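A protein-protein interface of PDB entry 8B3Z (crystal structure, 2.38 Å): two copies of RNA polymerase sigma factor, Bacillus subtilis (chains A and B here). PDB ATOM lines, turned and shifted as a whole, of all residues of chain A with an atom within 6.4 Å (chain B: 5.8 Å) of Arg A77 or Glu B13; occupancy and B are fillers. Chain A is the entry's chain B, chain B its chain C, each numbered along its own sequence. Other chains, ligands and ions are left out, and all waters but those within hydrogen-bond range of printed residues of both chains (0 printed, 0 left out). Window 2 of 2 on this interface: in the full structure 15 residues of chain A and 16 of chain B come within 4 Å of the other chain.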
ATOM      1  N   ILE A  39       9.586 -10.178 -17.769  1.00  0.00           N
ATOM      2  CA  ILE A  39       8.310 -10.362 -18.458  1.00  0.00           C
ATOM      3  C   ILE A  39       8.338 -11.632 -19.297  1.00  0.00           C
ATOM      4  O   ILE A  39       7.400 -12.440 -19.270  1.00  0.00           O
ATOM      5  CB  ILE A  39       7.993  -9.133 -19.331  1.00  0.00           C
ATOM      6  CG1 ILE A  39       7.743  -7.884 -18.471  1.00  0.00           C
ATOM      7  CG2 ILE A  39       6.821  -9.435 -20.268  1.00  0.00           C
ATOM      8  CD1 ILE A  39       6.586  -8.003 -17.492  1.00  0.00           C
ATOM      9  N   ILE A  42       7.931 -14.731 -17.400  1.00  0.00           N
ATOM     10  CA  ILE A  42       6.534 -14.987 -17.069  1.00  0.00           C
ATOM     11  C   ILE A  42       5.861 -15.770 -18.189  1.00  0.00           C
ATOM     12  O   ILE A  42       5.072 -16.690 -17.936  1.00  0.00           O
ATOM     13  CB  ILE A  42       5.819 -13.659 -16.769  1.00  0.00           C
ATOM     14  CG1 ILE A  42       6.421 -13.035 -15.507  1.00  0.00           C
ATOM     15  CG2 ILE A  42       4.305 -13.855 -16.668  1.00  0.00           C
ATOM     16  CD1 ILE A  42       5.901 -11.648 -15.213  1.00  0.00           C
ATOM     17  N   GLU A  70       3.794 -12.556 -24.169  1.00  0.00           N
ATOM     18  CA  GLU A  70       3.885 -11.833 -22.904  1.00  0.00           C
ATOM     19  C   GLU A  70       4.578 -10.488 -23.084  1.00  0.00           C
ATOM     20  O   GLU A  70       4.123  -9.471 -22.548  1.00  0.00           O
ATOM     21  CB  GLU A  70       4.621 -12.676 -21.865  1.00  0.00           C
ATOM     22  CG  GLU A  70       4.296 -12.297 -20.421  1.00  0.00           C
ATOM     23  CD  GLU A  70       2.864 -12.634 -20.023  1.00  0.00           C
ATOM     24  OE1 GLU A  70       2.222 -13.451 -20.716  1.00  0.00           O
ATOM     25  OE2 GLU A  70       2.380 -12.084 -19.013  1.00  0.00           O
ATOM     26  N   LEU A  72       4.952  -8.673 -25.942  1.00  0.00           N
ATOM     27  CA  LEU A  72       4.146  -7.763 -26.754  1.00  0.00           C
ATOM     28  C   LEU A  72       3.018  -7.141 -25.936  1.00  0.00           C
ATOM     29  O   LEU A  72       2.735  -5.944 -26.069  1.00  0.00           O
ATOM     30  CB  LEU A  72       3.579  -8.497 -27.971  1.00  0.00           C
ATOM     31  CG  LEU A  72       4.597  -9.017 -28.992  1.00  0.00           C
ATOM     32  CD1 LEU A  72       3.959 -10.037 -29.925  1.00  0.00           C
ATOM     33  CD2 LEU A  72       5.194  -7.879 -29.796  1.00  0.00           C
ATOM     34  N   MET A  73       2.367  -7.930 -25.078  1.00  0.00           N
ATOM     35  CA  MET A  73       1.281  -7.363 -24.282  1.00  0.00           C
ATOM     36  C   MET A  73       1.801  -6.367 -23.252  1.00  0.00           C
ATOM     37  O   MET A  73       1.123  -5.380 -22.945  1.00  0.00           O
ATOM     38  CB  MET A  73       0.470  -8.478 -23.619  1.00  0.00           C
ATOM     39  CG  MET A  73      -0.220  -9.412 -24.623  1.00  0.00           C
ATOM     40  SD  MET A  73      -1.070  -8.593 -26.015  1.00  0.00           S
ATOM     41  CE  MET A  73      -2.078  -7.338 -25.219  1.00  0.00           C
ATOM     42  N   TYR A  74       3.003  -6.594 -22.725  1.00  0.00           N
ATOM     43  CA  TYR A  74       3.635  -5.611 -21.854  1.00  0.00           C
ATOM     44  C   TYR A  74       3.955  -4.330 -22.618  1.00  0.00           C
ATOM     45  O   TYR A  74       3.716  -3.224 -22.121  1.00  0.00           O
ATOM     46  CB  TYR A  74       4.896  -6.222 -21.244  1.00  0.00           C
ATOM     47  CG  TYR A  74       5.736  -5.312 -20.383  1.00  0.00           C
ATOM     48  CD1 TYR A  74       5.387  -5.055 -19.058  1.00  0.00           C
ATOM     49  CD2 TYR A  74       6.909  -4.753 -20.874  1.00  0.00           C
ATOM     50  CE1 TYR A  74       6.171  -4.242 -18.258  1.00  0.00           C
ATOM     51  CE2 TYR A  74       7.702  -3.941 -20.083  1.00  0.00           C
ATOM     52  CZ  TYR A  74       7.330  -3.685 -18.777  1.00  0.00           C
ATOM     53  OH  TYR A  74       8.124  -2.866 -17.996  1.00  0.00           O
ATOM     54  N   LEU A  75       4.470  -4.465 -23.843  1.00  0.00           N
ATOM     55  CA  LEU A  75       4.818  -3.298 -24.647  1.00  0.00           C
ATOM     56  C   LEU A  75       3.579  -2.496 -25.033  1.00  0.00           C
ATOM     57  O   LEU A  75       3.621  -1.260 -25.073  1.00  0.00           O
ATOM     58  CB  LEU A  75       5.585  -3.748 -25.889  1.00  0.00           C
ATOM     59  CG  LEU A  75       7.041  -4.139 -25.623  1.00  0.00           C
ATOM     60  CD1 LEU A  75       7.867  -4.104 -26.898  1.00  0.00           C
ATOM     61  CD2 LEU A  75       7.658  -3.231 -24.572  1.00  0.00           C
ATOM     62  N   ARG A  76       2.465  -3.177 -25.323  1.00  0.00           N
ATOM     63  CA  ARG A  76       1.234  -2.463 -25.649  1.00  0.00           C
ATOM     64  C   ARG A  76       0.627  -1.819 -24.409  1.00  0.00           C
ATOM     65  O   ARG A  76       0.094  -0.706 -24.482  1.00  0.00           O
ATOM     66  CB  ARG A  76       0.226  -3.405 -26.309  1.00  0.00           C
ATOM     67  N   ARG A  77       0.704  -2.497 -23.260  1.00  0.00           N
ATOM     68  CA  ARG A  77       0.177  -1.920 -22.027  1.00  0.00           C
ATOM     69  C   ARG A  77       0.911  -0.638 -21.659  1.00  0.00           C
ATOM     70  O   ARG A  77       0.300   0.315 -21.161  1.00  0.00           O
ATOM     71  CB  ARG A  77       0.273  -2.928 -20.885  1.00  0.00           C
ATOM     72  CG  ARG A  77      -0.939  -3.828 -20.740  1.00  0.00           C
ATOM     73  CD  ARG A  77      -0.987  -4.443 -19.349  1.00  0.00           C
ATOM     74  NE  ARG A  77       0.303  -5.011 -18.960  1.00  0.00           N
ATOM     75  CZ  ARG A  77       0.705  -6.239 -19.276  1.00  0.00           C
ATOM     76  NH1 ARG A  77      -0.081  -7.031 -19.992  1.00  0.00           N
ATOM     77  NH2 ARG A  77       1.893  -6.675 -18.882  1.00  0.00           N
ATOM     78  N   ASN A  78       2.221  -0.595 -21.899  1.00  0.00           N
ATOM     79  CA  ASN A  78       3.042   0.572 -21.600  1.00  0.00           C
ATOM     80  C   ASN A  78       3.384   1.374 -22.851  1.00  0.00           C
ATOM     81  O   ASN A  78       4.424   2.041 -22.892  1.00  0.00           O
ATOM     82  CB  ASN A  78       4.316   0.140 -20.877  1.00  0.00           C
ATOM     83  CG  ASN A  78       4.026  -0.673 -19.631  1.00  0.00           C
ATOM     84  OD1 ASN A  78       2.933  -0.602 -19.069  1.00  0.00           O
ATOM     85  ND2 ASN A  78       5.001  -1.462 -19.203  1.00  0.00           N
ATOM     86  N   ASN A  79       2.526   1.318 -23.869  1.00  0.00           N
ATOM     87  CA  ASN A  79       2.732   2.037 -25.125  1.00  0.00           C
ATOM     88  C   ASN A  79       4.109   1.757 -25.728  1.00  0.00           C
ATOM     89  O   ASN A  79       4.233   1.035 -26.719  1.00  0.00           O
ATOM     90  CB  ASN A  79       2.548   3.539 -24.916  1.00  0.00           C
ATOM     91  N   ARG B   8      -2.704  -9.169  -9.003  1.00  0.00           N
ATOM     92  CA  ARG B   8      -1.410  -9.839  -8.962  1.00  0.00           C
ATOM     93  C   ARG B   8      -0.465  -9.284 -10.021  1.00  0.00           C
ATOM     94  O   ARG B   8       0.714  -9.050  -9.729  1.00  0.00           O
ATOM     95  CB  ARG B   8      -1.598 -11.349  -9.135  1.00  0.00           C
ATOM     96  CG  ARG B   8      -2.222 -12.018  -7.912  1.00  0.00           C
ATOM     97  CD  ARG B   8      -2.919 -13.331  -8.285  1.00  0.00           C
ATOM     98  NE  ARG B   8      -3.656 -13.241  -9.546  1.00  0.00           N
ATOM     99  CZ  ARG B   8      -4.798 -12.577  -9.712  1.00  0.00           C
ATOM    100  NH1 ARG B   8      -5.365 -11.934  -8.692  1.00  0.00           N
ATOM    101  NH2 ARG B   8      -5.377 -12.563 -10.907  1.00  0.00           N
ATOM    102  N   ALA B   9      -0.967  -9.060 -11.238  1.00  0.00           N
ATOM    103  CA  ALA B   9      -0.110  -8.542 -12.299  1.00  0.00           C
ATOM    104  C   ALA B   9       0.418  -7.149 -11.969  1.00  0.00           C
ATOM    105  O   ALA B   9       1.501  -6.766 -12.434  1.00  0.00           O
ATOM    106  CB  ALA B   9      -0.875  -8.529 -13.620  1.00  0.00           C
ATOM    107  N   ILE B  10      -0.340  -6.371 -11.193  1.00  0.00           N
ATOM    108  CA  ILE B  10       0.154  -5.079 -10.718  1.00  0.00           C
ATOM    109  C   ILE B  10       1.330  -5.283  -9.772  1.00  0.00           C
ATOM    110  O   ILE B  10       2.385  -4.654  -9.916  1.00  0.00           O
ATOM    111  CB  ILE B  10      -0.980  -4.289 -10.040  1.00  0.00           C
ATOM    112  CG1 ILE B  10      -2.048  -3.897 -11.065  1.00  0.00           C
ATOM    113  CG2 ILE B  10      -0.428  -3.058  -9.327  1.00  0.00           C
ATOM    114  CD1 ILE B  10      -1.545  -2.967 -12.143  1.00  0.00           C
ATOM    115  N   LEU B  11       1.161  -6.174  -8.789  1.00  0.00           N
ATOM    116  CA  LEU B  11       2.214  -6.431  -7.809  1.00  0.00           C
ATOM    117  C   LEU B  11       3.484  -6.951  -8.469  1.00  0.00           C
ATOM    118  O   LEU B  11       4.595  -6.590  -8.063  1.00  0.00           O
ATOM    119  CB  LEU B  11       1.723  -7.432  -6.764  1.00  0.00           C
ATOM    120  CG  LEU B  11       0.682  -6.921  -5.775  1.00  0.00           C
ATOM    121  CD1 LEU B  11       0.091  -8.082  -4.996  1.00  0.00           C
ATOM    122  CD2 LEU B  11       1.296  -5.889  -4.837  1.00  0.00           C
ATOM    123  N   ILE B  12       3.347  -7.806  -9.480  1.00  0.00           N
ATOM    124  CA  ILE B  12       4.531  -8.355 -10.132  1.00  0.00           C
ATOM    125  C   ILE B  12       5.256  -7.272 -10.915  1.00  0.00           C
ATOM    126  O   ILE B  12       6.467  -7.085 -10.764  1.00  0.00           O
ATOM    127  CB  ILE B  12       4.156  -9.541 -11.034  1.00  0.00           C
ATOM    128  CG1 ILE B  12       3.697 -10.729 -10.187  1.00  0.00           C
ATOM    129  CG2 ILE B  12       5.337  -9.929 -11.903  1.00  0.00           C
ATOM    130  CD1 ILE B  12       3.038 -11.818 -10.992  1.00  0.00           C
ATOM    131  N   GLU B  13       4.527  -6.542 -11.766  1.00  0.00           N
ATOM    132  CA  GLU B  13       5.169  -5.524 -12.590  1.00  0.00           C
ATOM    133  C   GLU B  13       5.762  -4.413 -11.742  1.00  0.00           C
ATOM    134  O   GLU B  13       6.776  -3.816 -12.119  1.00  0.00           O
ATOM    135  CB  GLU B  13       4.177  -4.942 -13.597  1.00  0.00           C
ATOM    136  CG  GLU B  13       3.805  -5.887 -14.724  1.00  0.00           C
ATOM    137  CD  GLU B  13       3.141  -5.180 -15.894  1.00  0.00           C
ATOM    138  OE1 GLU B  13       3.372  -3.965 -16.079  1.00  0.00           O
ATOM    139  OE2 GLU B  13       2.374  -5.842 -16.626  1.00  0.00           O
ATOM    140  N   ARG B  14       5.158  -4.128 -10.594  1.00  0.00           N
ATOM    141  CA  ARG B  14       5.649  -3.050  -9.753  1.00  0.00           C
ATOM    142  C   ARG B  14       6.920  -3.427  -9.007  1.00  0.00           C
ATOM    143  O   ARG B  14       7.604  -2.535  -8.493  1.00  0.00           O
ATOM    144  CB  ARG B  14       4.554  -2.626  -8.766  1.00  0.00           C
ATOM    145  CG  ARG B  14       4.799  -1.298  -8.077  1.00  0.00           C
ATOM    146  CD  ARG B  14       3.503  -0.688  -7.577  1.00  0.00           C
ATOM    147  NE  ARG B  14       2.714  -0.117  -8.663  1.00  0.00           N
ATOM    148  CZ  ARG B  14       1.541   0.486  -8.495  1.00  0.00           C
ATOM    149  NH1 ARG B  14       1.020   0.595  -7.280  1.00  0.00           N
ATOM    150  NH2 ARG B  14       0.891   0.985  -9.538  1.00  0.00           N
ATOM    151  N   ASN B  15       7.261  -4.716  -8.947  1.00  0.00           N
ATOM    152  CA  ASN B  15       8.424  -5.174  -8.198  1.00  0.00           C
ATOM    153  C   ASN B  15       9.441  -5.907  -9.068  1.00  0.00           C
ATOM    154  O   ASN B  15      10.223  -6.709  -8.553  1.00  0.00           O
ATOM    155  CB  ASN B  15       7.992  -6.057  -7.027  1.00  0.00           C
ATOM    156  CG  ASN B  15       7.357  -5.255  -5.905  1.00  0.00           C
ATOM    157  OD1 ASN B  15       7.171  -4.037  -6.017  1.00  0.00           O
ATOM    158  ND2 ASN B  15       7.036  -5.932  -4.807  1.00  0.00           N
ATOM    159  N   LEU B  16       9.459  -5.644 -10.375  1.00  0.00           N
ATOM    160  CA  LEU B  16      10.485  -6.250 -11.220  1.00  0.00           C
ATOM    161  C   LEU B  16      11.871  -5.760 -10.829  1.00  0.00           C
ATOM    162  O   LEU B  16      12.844  -6.523 -10.875  1.00  0.00           O
ATOM    163  CB  LEU B  16      10.213  -5.947 -12.690  1.00  0.00           C
ATOM    164  CG  LEU B  16       8.904  -6.508 -13.239  1.00  0.00           C
ATOM    165  CD1 LEU B  16       8.872  -6.373 -14.755  1.00  0.00           C
ATOM    166  CD2 LEU B  16       8.720  -7.950 -12.811  1.00  0.00           C
ATOM    167  N   ARG B  17      11.980  -4.484 -10.445  1.00  0.00           N
ATOM    168  CA  ARG B  17      13.275  -3.941 -10.056  1.00  0.00           C
ATOM    169  C   ARG B  17      13.838  -4.672  -8.850  1.00  0.00           C
ATOM    170  O   ARG B  17      15.056  -4.862  -8.754  1.00  0.00           O
ATOM    171  CB  ARG B  17      13.162  -2.443  -9.760  1.00  0.00           C
ATOM    172  CG  ARG B  17      12.882  -1.586 -10.982  1.00  0.00           C
ATOM    173  CD  ARG B  17      13.954  -1.768 -12.055  1.00  0.00           C
ATOM    174  NE  ARG B  17      15.236  -1.192 -11.653  1.00  0.00           N
ATOM    175  CZ  ARG B  17      16.410  -1.534 -12.174  1.00  0.00           C
ATOM    176  NH1 ARG B  17      16.474  -2.451 -13.127  1.00  0.00           N
ATOM    177  NH2 ARG B  17      17.519  -0.947 -11.750  1.00  0.00           N
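NH2 of Arg A77 lies within salt-bridge range of OE2 of Glu B13, 2.5 Å away.
Among the printed residues, merely in contact across the chains: Tyr A74 with Glu B13, Ile A42 with Ile B12 and Ile A39 with Leu B16.
Of chain A, only Tyr A74 and Arg A77 come within 4 Å of Glu B13. Printed residues of chain A within 4 Å of Leu B16: Ile A39. Printed residues of chain B within 4 Å of Ile A42: Ile B12. Printed residues of chain B within 4 Å of Tyr A74: Glu B13 (3.6 Å). The nearest residue of chain A that does not touch Glu B13 is Asn A78 (4.3 Å). The nearest printed residue of chain B that does not touch Tyr A74 is Leu B16 (4.8 Å).
Of the 10 printed residues of chain B, 3 touch a printed residue of chain A. Hydrophobic or aromatic side chains of chain B that line the printed part of chain A: Ile B12 and Leu B16. Printed residues of chain A that touch a printed residue of chain B: Ile A39, Ile A42, Tyr A74 and Arg A77. Hydrophobic or aromatic side chains of chain A that line the printed part of chain B: Ile A39, Ile A42 and Tyr A74.
No position is printed for both chains. Of the 4 pairs that touch across the chains among the printed residues, none has its exchanged pair printed and touching as well.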
